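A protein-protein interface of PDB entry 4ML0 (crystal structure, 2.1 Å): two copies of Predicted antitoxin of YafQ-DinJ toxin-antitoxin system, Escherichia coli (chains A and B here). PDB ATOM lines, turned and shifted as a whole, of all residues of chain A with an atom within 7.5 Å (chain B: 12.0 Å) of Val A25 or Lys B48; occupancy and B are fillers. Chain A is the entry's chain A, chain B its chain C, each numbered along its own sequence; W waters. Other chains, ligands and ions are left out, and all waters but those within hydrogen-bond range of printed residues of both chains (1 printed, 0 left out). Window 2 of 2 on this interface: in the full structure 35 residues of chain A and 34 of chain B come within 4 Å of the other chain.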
ATOM      1  N   LYS A  19     -19.225  -8.909 -21.903  1.00  0.00           N
ATOM      2  CA  LYS A  19     -20.546  -8.381 -21.542  1.00  0.00           C
ATOM      3  C   LYS A  19     -21.676  -9.294 -22.012  1.00  0.00           C
ATOM      4  O   LYS A  19     -22.562  -9.648 -21.227  1.00  0.00           O
ATOM      5  CB  LYS A  19     -20.755  -6.964 -22.112  1.00  0.00           C
ATOM      6  CG  LYS A  19     -22.129  -6.346 -21.791  1.00  0.00           C
ATOM      7  CD  LYS A  19     -22.309  -4.960 -22.436  1.00  0.00           C
ATOM      8  CE  LYS A  19     -23.647  -4.320 -22.035  1.00  0.00           C
ATOM      9  NZ  LYS A  19     -23.953  -3.086 -22.842  1.00  0.00           N
ATOM     10  N   ASN A  20     -21.654  -9.679 -23.287  1.00  0.00           N
ATOM     11  CA  ASN A  20     -22.688 -10.574 -23.805  1.00  0.00           C
ATOM     12  C   ASN A  20     -22.725 -11.921 -23.080  1.00  0.00           C
ATOM     13  O   ASN A  20     -23.803 -12.446 -22.767  1.00  0.00           O
ATOM     14  CB  ASN A  20     -22.516 -10.810 -25.313  1.00  0.00           C
ATOM     15  CG  ASN A  20     -22.768  -9.560 -26.140  1.00  0.00           C
ATOM     16  OD1 ASN A  20     -23.458  -8.631 -25.703  1.00  0.00           O
ATOM     17  ND2 ASN A  20     -22.214  -9.534 -27.352  1.00  0.00           N
ATOM     18  N   GLN A  21     -21.551 -12.490 -22.816  1.00  0.00           N
ATOM     19  CA  GLN A  21     -21.523 -13.793 -22.149  1.00  0.00           C
ATOM     20  C   GLN A  21     -22.059 -13.720 -20.711  1.00  0.00           C
ATOM     21  O   GLN A  21     -22.883 -14.549 -20.296  1.00  0.00           O
ATOM     22  CB  GLN A  21     -20.122 -14.423 -22.186  1.00  0.00           C
ATOM     23  CG  GLN A  21     -20.123 -15.902 -21.786  1.00  0.00           C
ATOM     24  CD  GLN A  21     -18.795 -16.579 -22.061  1.00  0.00           C
ATOM     25  OE1 GLN A  21     -18.366 -16.680 -23.211  1.00  0.00           O
ATOM     26  NE2 GLN A  21     -18.127 -17.031 -20.999  1.00  0.00           N
ATOM     27  N   ALA A  22     -21.594 -12.730 -19.956  1.00  0.00           N
ATOM     28  CA  ALA A  22     -22.077 -12.529 -18.590  1.00  0.00           C
ATOM     29  C   ALA A  22     -23.576 -12.291 -18.602  1.00  0.00           C
ATOM     30  O   ALA A  22     -24.303 -12.786 -17.741  1.00  0.00           O
ATOM     31  CB  ALA A  22     -21.370 -11.330 -17.936  1.00  0.00           C
ATOM     32  N   ALA A  23     -24.037 -11.500 -19.568  1.00  0.00           N
ATOM     33  CA  ALA A  23     -25.466 -11.230 -19.689  1.00  0.00           C
ATOM     34  C   ALA A  23     -26.242 -12.520 -19.942  1.00  0.00           C
ATOM     35  O   ALA A  23     -27.311 -12.705 -19.368  1.00  0.00           O
ATOM     36  CB  ALA A  23     -25.749 -10.182 -20.781  1.00  0.00           C
ATOM     37  N   ASP A  24     -25.713 -13.421 -20.779  1.00  0.00           N
ATOM     38  CA  ASP A  24     -26.364 -14.736 -20.990  1.00  0.00           C
ATOM     39  C   ASP A  24     -26.444 -15.584 -19.711  1.00  0.00           C
ATOM     40  O   ASP A  24     -27.516 -16.162 -19.355  1.00  0.00           O
ATOM     41  CB  ASP A  24     -25.600 -15.555 -22.036  1.00  0.00           C
ATOM     42  CG  ASP A  24     -25.682 -14.961 -23.423  1.00  0.00           C
ATOM     43  OD1 ASP A  24     -26.725 -14.354 -23.748  1.00  0.00           O
ATOM     44  OD2 ASP A  24     -24.697 -15.107 -24.188  1.00  0.00           O
ATOM     45  N   VAL A  25     -25.298 -15.678 -19.034  1.00  0.00           N
ATOM     46  CA  VAL A  25     -25.234 -16.413 -17.771  1.00  0.00           C
ATOM     47  C   VAL A  25     -26.286 -15.873 -16.801  1.00  0.00           C
ATOM     48  O   VAL A  25     -27.049 -16.633 -16.206  1.00  0.00           O
ATOM     49  CB  VAL A  25     -23.831 -16.307 -17.126  1.00  0.00           C
ATOM     50  CG1 VAL A  25     -23.847 -16.863 -15.710  1.00  0.00           C
ATOM     51  CG2 VAL A  25     -22.801 -17.043 -17.980  1.00  0.00           C
ATOM     52  N   LEU A  26     -26.339 -14.554 -16.665  1.00  0.00           N
ATOM     53  CA  LEU A  26     -27.258 -13.916 -15.709  1.00  0.00           C
ATOM     54  C   LEU A  26     -28.728 -14.077 -16.107  1.00  0.00           C
ATOM     55  O   LEU A  26     -29.609 -14.294 -15.251  1.00  0.00           O
ATOM     56  CB  LEU A  26     -26.904 -12.433 -15.551  1.00  0.00           C
ATOM     57  CG  LEU A  26     -25.555 -12.193 -14.861  1.00  0.00           C
ATOM     58  CD1 LEU A  26     -25.154 -10.719 -14.932  1.00  0.00           C
ATOM     59  CD2 LEU A  26     -25.567 -12.672 -13.399  1.00  0.00           C
ATOM     60  N   ALA A  27     -28.989 -13.976 -17.407  1.00  0.00           N
ATOM     61  CA  ALA A  27     -30.353 -14.091 -17.930  1.00  0.00           C
ATOM     62  C   ALA A  27     -30.881 -15.468 -17.589  1.00  0.00           C
ATOM     63  O   ALA A  27     -32.059 -15.623 -17.242  1.00  0.00           O
ATOM     64  CB  ALA A  27     -30.392 -13.864 -19.433  1.00  0.00           C
ATOM     65  N   GLY A  28     -30.008 -16.470 -17.665  1.00  0.00           N
ATOM     66  CA  GLY A  28     -30.410 -17.793 -17.196  1.00  0.00           C
ATOM     67  C   GLY A  28     -31.008 -17.843 -15.780  1.00  0.00           C
ATOM     68  O   GLY A  28     -31.760 -18.759 -15.446  1.00  0.00           O
ATOM     69  N   MET A  29     -30.678 -16.866 -14.940  1.00  0.00           N
ATOM     70  CA  MET A  29     -31.139 -16.864 -13.551  1.00  0.00           C
ATOM     71  C   MET A  29     -32.092 -15.716 -13.290  1.00  0.00           C
ATOM     72  O   MET A  29     -32.322 -15.351 -12.138  1.00  0.00           O
ATOM     73  CB  MET A  29     -29.958 -16.721 -12.587  1.00  0.00           C
ATOM     74  CG  MET A  29     -28.850 -17.714 -12.787  1.00  0.00           C
ATOM     75  SD  MET A  29     -27.619 -17.556 -11.472  1.00  0.00           S
ATOM     76  CE  MET A  29     -26.394 -18.744 -12.076  1.00  0.00           C
ATOM     77  N   GLY A  30     -32.626 -15.125 -14.349  1.00  0.00           N
ATOM     78  CA  GLY A  30     -33.608 -14.069 -14.181  1.00  0.00           C
ATOM     79  C   GLY A  30     -33.009 -12.724 -13.796  1.00  0.00           C
ATOM     80  O   GLY A  30     -33.741 -11.803 -13.407  1.00  0.00           O
ATOM     81  N   LEU A  31     -31.688 -12.595 -13.920  1.00  0.00           N
ATOM     82  CA  LEU A  31     -31.017 -11.343 -13.581  1.00  0.00           C
ATOM     83  C   LEU A  31     -30.497 -10.619 -14.819  1.00  0.00           C
ATOM     84  O   LEU A  31     -30.178 -11.254 -15.828  1.00  0.00           O
ATOM     85  CB  LEU A  31     -29.869 -11.614 -12.613  1.00  0.00           C
ATOM     86  CG  LEU A  31     -30.254 -12.195 -11.259  1.00  0.00           C
ATOM     87  CD1 LEU A  31     -29.017 -12.696 -10.548  1.00  0.00           C
ATOM     88  CD2 LEU A  31     -30.964 -11.155 -10.404  1.00  0.00           C
ATOM     89  N   ILE B  39     -14.303  -6.869 -12.891  1.00  0.00           N
ATOM     90  CA  ILE B  39     -13.868  -8.055 -12.146  1.00  0.00           C
ATOM     91  C   ILE B  39     -15.025  -9.037 -11.897  1.00  0.00           C
ATOM     92  O   ILE B  39     -14.910 -10.261 -12.129  1.00  0.00           O
ATOM     93  CB  ILE B  39     -13.232  -7.607 -10.806  1.00  0.00           C
ATOM     94  CG1 ILE B  39     -11.909  -6.887 -11.086  1.00  0.00           C
ATOM     95  CG2 ILE B  39     -13.007  -8.778  -9.864  1.00  0.00           C
ATOM     96  CD1 ILE B  39     -11.342  -6.135  -9.877  1.00  0.00           C
ATOM     97  N   THR B  40     -16.154  -8.502 -11.430  1.00  0.00           N
ATOM     98  CA  THR B  40     -17.307  -9.340 -11.111  1.00  0.00           C
ATOM     99  C   THR B  40     -17.922  -9.978 -12.368  1.00  0.00           C
ATOM    100  O   THR B  40     -18.261 -11.163 -12.366  1.00  0.00           O
ATOM    101  CB  THR B  40     -18.384  -8.529 -10.363  1.00  0.00           C
ATOM    102  OG1 THR B  40     -17.799  -7.967  -9.189  1.00  0.00           O
ATOM    103  CG2 THR B  40     -19.539  -9.420  -9.936  1.00  0.00           C
ATOM    104  N   LEU B  41     -18.077  -9.197 -13.436  1.00  0.00           N
ATOM    105  CA  LEU B  41     -18.645  -9.746 -14.664  1.00  0.00           C
ATOM    106  C   LEU B  41     -17.703 -10.795 -15.261  1.00  0.00           C
ATOM    107  O   LEU B  41     -18.144 -11.804 -15.812  1.00  0.00           O
ATOM    108  CB  LEU B  41     -18.967  -8.624 -15.663  1.00  0.00           C
ATOM    109  CG  LEU B  41     -20.165  -7.765 -15.222  1.00  0.00           C
ATOM    110  CD1 LEU B  41     -20.471  -6.668 -16.221  1.00  0.00           C
ATOM    111  CD2 LEU B  41     -21.391  -8.636 -15.023  1.00  0.00           C
ATOM    112  N   THR B  42     -16.401 -10.575 -15.122  1.00  0.00           N
ATOM    113  CA  THR B  42     -15.431 -11.568 -15.596  1.00  0.00           C
ATOM    114  C   THR B  42     -15.598 -12.889 -14.843  1.00  0.00           C
ATOM    115  O   THR B  42     -15.601 -13.962 -15.452  1.00  0.00           O
ATOM    116  CB  THR B  42     -13.992 -11.057 -15.430  1.00  0.00           C
ATOM    117  OG1 THR B  42     -13.790  -9.932 -16.295  1.00  0.00           O
ATOM    118  CG2 THR B  42     -12.972 -12.159 -15.780  1.00  0.00           C
ATOM    119  N   LYS B  43     -15.721 -12.817 -13.517  1.00  0.00           N
ATOM    120  CA  LYS B  43     -15.920 -14.039 -12.738  1.00  0.00           C
ATOM    121  C   LYS B  43     -17.227 -14.737 -13.136  1.00  0.00           C
ATOM    122  O   LYS B  43     -17.248 -15.954 -13.352  1.00  0.00           O
ATOM    123  CB  LYS B  43     -15.911 -13.740 -11.235  1.00  0.00           C
ATOM    124  CG  LYS B  43     -16.049 -14.990 -10.360  1.00  0.00           C
ATOM    125  CD  LYS B  43     -16.067 -14.637  -8.864  1.00  0.00           C
ATOM    126  CE  LYS B  43     -16.341 -15.886  -8.000  1.00  0.00           C
ATOM    127  NZ  LYS B  43     -15.211 -16.855  -8.021  1.00  0.00           N
ATOM    128  N   VAL B  44     -18.313 -13.969 -13.247  1.00  0.00           N
ATOM    129  CA  VAL B  44     -19.588 -14.537 -13.704  1.00  0.00           C
ATOM    130  C   VAL B  44     -19.483 -15.220 -15.081  1.00  0.00           C
ATOM    131  O   VAL B  44     -19.960 -16.346 -15.257  1.00  0.00           O
ATOM    132  CB  VAL B  44     -20.711 -13.458 -13.710  1.00  0.00           C
ATOM    133  CG1 VAL B  44     -21.922 -13.939 -14.495  1.00  0.00           C
ATOM    134  CG2 VAL B  44     -21.101 -13.107 -12.276  1.00  0.00           C
ATOM    135  N   ALA B  45     -18.850 -14.548 -16.043  1.00  0.00           N
ATOM    136  CA  ALA B  45     -18.695 -15.100 -17.398  1.00  0.00           C
ATOM    137  C   ALA B  45     -17.866 -16.375 -17.400  1.00  0.00           C
ATOM    138  O   ALA B  45     -18.212 -17.345 -18.079  1.00  0.00           O
ATOM    139  CB  ALA B  45     -18.068 -14.086 -18.340  1.00  0.00           C
ATOM    140  N   ARG B  46     -16.755 -16.371 -16.669  1.00  0.00           N
ATOM    141  CA  ARG B  46     -15.891 -17.555 -16.672  1.00  0.00           C
ATOM    142  C   ARG B  46     -16.531 -18.735 -15.975  1.00  0.00           C
ATOM    143  O   ARG B  46     -16.414 -19.869 -16.437  1.00  0.00           O
ATOM    144  CB  ARG B  46     -14.551 -17.265 -15.999  1.00  0.00           C
ATOM    145  CG  ARG B  46     -13.678 -16.381 -16.825  1.00  0.00           C
ATOM    146  CD  ARG B  46     -12.355 -16.120 -16.142  1.00  0.00           C
ATOM    147  NE  ARG B  46     -11.536 -15.162 -16.899  1.00  0.00           N
ATOM    148  CZ  ARG B  46     -10.622 -14.384 -16.333  1.00  0.00           C
ATOM    149  NH1 ARG B  46     -10.440 -14.446 -15.006  1.00  0.00           N
ATOM    150  NH2 ARG B  46      -9.920 -13.533 -17.077  1.00  0.00           N
ATOM    151  N   GLU B  47     -17.184 -18.483 -14.844  1.00  0.00           N
ATOM    152  CA  GLU B  47     -17.664 -19.590 -14.027  1.00  0.00           C
ATOM    153  C   GLU B  47     -19.068 -20.014 -14.392  1.00  0.00           C
ATOM    154  O   GLU B  47     -19.506 -21.092 -14.004  1.00  0.00           O
ATOM    155  CB  GLU B  47     -17.575 -19.248 -12.535  1.00  0.00           C
ATOM    156  CG  GLU B  47     -16.146 -18.989 -12.095  1.00  0.00           C
ATOM    157  CD  GLU B  47     -16.035 -18.604 -10.617  1.00  0.00           C
ATOM    158  OE1 GLU B  47     -17.076 -18.582  -9.920  1.00  0.00           O
ATOM    159  OE2 GLU B  47     -14.904 -18.315 -10.160  1.00  0.00           O
ATOM    160  N   LYS B  48     -19.765 -19.176 -15.156  1.00  0.00           N
ATOM    161  CA  LYS B  48     -21.177 -19.420 -15.474  1.00  0.00           C
ATOM    162  C   LYS B  48     -21.944 -19.618 -14.169  1.00  0.00           C
ATOM    163  O   LYS B  48     -22.801 -20.496 -14.064  1.00  0.00           O
ATOM    164  CB  LYS B  48     -21.357 -20.655 -16.377  1.00  0.00           C
ATOM    165  CG  LYS B  48     -20.209 -20.887 -17.362  1.00  0.00           C
ATOM    166  CD  LYS B  48     -20.212 -19.873 -18.468  1.00  0.00           C
ATOM    167  CE  LYS B  48     -19.228 -20.270 -19.592  1.00  0.00           C
ATOM    168  NZ  LYS B  48     -17.787 -20.169 -19.205  1.00  0.00           N
ATOM    169  N   ALA B  49     -21.615 -18.804 -13.170  1.00  0.00           N
ATOM    170  CA  ALA B  49     -22.258 -18.889 -11.869  1.00  0.00           C
ATOM    171  C   ALA B  49     -22.126 -17.548 -11.154  1.00  0.00           C
ATOM    172  O   ALA B  49     -21.341 -16.690 -11.563  1.00  0.00           O
ATOM    173  CB  ALA B  49     -21.632 -19.999 -11.044  1.00  0.00           C
ATOM    174  N   LEU B  50     -22.879 -17.379 -10.077  1.00  0.00           N
ATOM    175  CA  LEU B  50     -22.809 -16.161  -9.285  1.00  0.00           C
ATOM    176  C   LEU B  50     -21.727 -16.306  -8.228  1.00  0.00           C
ATOM    177  O   LEU B  50     -21.483 -17.410  -7.747  1.00  0.00           O
ATOM    178  CB  LEU B  50     -24.148 -15.938  -8.578  1.00  0.00           C
ATOM    179  CG  LEU B  50     -25.085 -14.843  -9.063  1.00  0.00           C
ATOM    180  CD1 LEU B  50     -25.236 -14.906 -10.560  1.00  0.00           C
ATOM    181  CD2 LEU B  50     -26.447 -14.976  -8.380  1.00  0.00           C
ATOM    182  N   PRO B  51     -21.081 -15.194  -7.844  1.00  0.00           N
ATOM    183  CA  PRO B  51     -20.229 -15.202  -6.642  1.00  0.00           C
ATOM    184  C   PRO B  51     -21.071 -15.603  -5.416  1.00  0.00           C
ATOM    185  O   PRO B  51     -22.300 -15.447  -5.476  1.00  0.00           O
ATOM    186  CB  PRO B  51     -19.801 -13.737  -6.506  1.00  0.00           C
ATOM    187  CG  PRO B  51     -19.935 -13.160  -7.909  1.00  0.00           C
ATOM    188  CD  PRO B  51     -21.121 -13.876  -8.507  1.00  0.00           C
ATOM    189  N   PHE B  52     -20.439 -16.092  -4.340  1.00  0.00           N
ATOM    190  CA  PHE B  52     -21.172 -16.589  -3.159  1.00  0.00           C
ATOM    191  C   PHE B  52     -21.783 -15.458  -2.354  1.00  0.00           C
ATOM    192  O   PHE B  52     -21.283 -14.337  -2.382  1.00  0.00           O
ATOM    193  CB  PHE B  52     -20.244 -17.351  -2.195  1.00  0.00           C
ATOM    194  CG  PHE B  52     -19.715 -18.664  -2.726  1.00  0.00           C
ATOM    195  CD1 PHE B  52     -20.337 -19.318  -3.780  1.00  0.00           C
ATOM    196  CD2 PHE B  52     -18.585 -19.245  -2.146  1.00  0.00           C
ATOM    197  CE1 PHE B  52     -19.834 -20.537  -4.262  1.00  0.00           C
ATOM    198  CE2 PHE B  52     -18.083 -20.461  -2.608  1.00  0.00           C
ATOM    199  CZ  PHE B  52     -18.702 -21.107  -3.668  1.00  0.00           C
ATOM    200  N   LEU B  54     -24.102 -13.275  -2.231  1.00  0.00           N
ATOM    201  CA  LEU B  54     -24.409 -11.916  -2.687  1.00  0.00           C
ATOM    202  C   LEU B  54     -25.626 -11.345  -1.955  1.00  0.00           C
ATOM    203  O   LEU B  54     -25.711 -10.133  -1.717  1.00  0.00           O
ATOM    204  CB  LEU B  54     -24.622 -11.867  -4.199  1.00  0.00           C
ATOM    205  CG  LEU B  54     -23.380 -11.957  -5.091  1.00  0.00           C
ATOM    206  CD1 LEU B  54     -23.813 -11.928  -6.519  1.00  0.00           C
ATOM    207  CD2 LEU B  54     -22.396 -10.819  -4.844  1.00  0.00           C
ATOM    208  N   ARG B  55     -26.561 -12.223  -1.588  1.00  0.00           N
ATOM    209  CA  ARG B  55     -27.794 -11.811  -0.902  1.00  0.00           C
ATOM    210  C   ARG B  55     -28.036 -12.674   0.334  1.00  0.00           C
ATOM    211  O   ARG B  55     -27.762 -13.876   0.323  1.00  0.00           O
ATOM    212  CB  ARG B  55     -29.002 -11.893  -1.862  1.00  0.00           C
ATOM    213  CG  ARG B  55     -28.977 -10.881  -3.008  1.00  0.00           C
ATOM    214  CD  ARG B  55     -30.028 -11.158  -4.103  1.00  0.00           C
ATOM    215  NE  ARG B  55     -29.717 -12.345  -4.917  1.00  0.00           N
ATOM    216  CZ  ARG B  55     -30.504 -12.827  -5.880  1.00  0.00           C
ATOM    217  NH1 ARG B  55     -31.656 -12.223  -6.168  1.00  0.00           N
ATOM    218  NH2 ARG B  55     -30.139 -13.906  -6.564  1.00  0.00           N
HETATM  219  O   HOH W   1     -31.349 -15.062  -9.159  1.00  0.00           O
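The backbone carbonyl oxygen of Ala B45 sits at hydrogen-bond distance from the side-chain amide nitrogen of Gln A21, at 2.9 Å.
O of Leu A26 is in hydrogen-bond range of N of Leu A31 (3.0 Å). The backbone carbonyl oxygen (O) of Ala B45 is in hydrogen-bond range of the side-chain amino group (NZ) of Lys B48, at 3.1 Å. The backbone carbonyl oxygen (O) of Arg B46 sits at hydrogen-bond distance from the side-chain amino group (NZ) of Lys B48.
NZ of Lys B48 touches NE2 of Gln A21, at 3.6 Å. Leu B41 touches Ala A22. CG1 of Val A25 touches CG1 of Val B44 (3.7 Å). Val A25 touches Lys B48 (CG1 to C, 3.7 Å). Ala B49 touches Val A25 (N to CG1, 3.9 Å). Leu A26 touches Leu B50 (CD2 to CD1, 3.6 Å). Leu B50 touches Met A29 (CD1 to SD, 3.7 Å).
Gln A21 touches just these residues of chain B: Ala B45 (2.9 Å) and Lys B48 (3.6 Å). Ala A22 touches one residue of chain B. No residue of chain B comes within 4 Å of Asp A24. Of the printed residues of chain B, Val A25 touches Val B44 (3.7 Å), Lys B48 (3.7 Å) and Ala B49 (3.9 Å). No residue of chain B comes within 4 Å of Ala A27. No residue of chain B comes within 4 Å of Gly A28. Met A29 touches just one residue of chain B: Leu B50. Printed residues of chain A within 4 Å of Val B44: Val A25. Printed residues of chain A within 4 Å of Lys B48: Gln A21 and Val A25. Printed residues of chain A within 4 Å of Ala B49: Val A25 (3.9 Å). The nearest residue of chain B that does not touch Val A25 is Ala B45 (4.6 Å).
Of the 13 printed residues of chain A, 5 touch a printed residue of chain B. Hydrophobic or aromatic side chains of chain A within 4 Å of the printed part of chain B: Ala A22, Val A25, Leu A26 and Met A29. Along chain A the printed residues that touch a printed residue of chain B span positions 21 to 29. Of the 16 printed residues of chain B, 6 touch a printed residue of chain A. Among the printed residues, no Asp or Glu carboxylate lies within 4 Å of a Lys or Arg side-chain nitrogen of the other chain.
No position is printed for both chains. Of the 8 pairs that touch across the chains among the printed residues, none has its exchanged pair printed and touching as well.
Water W1 lies within hydrogen-bond range of the guanidinium group (NH2) of Arg B55 (3.1 Å) and the backbone carbonyl oxygen (O) of Met A29 (3.1 Å).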
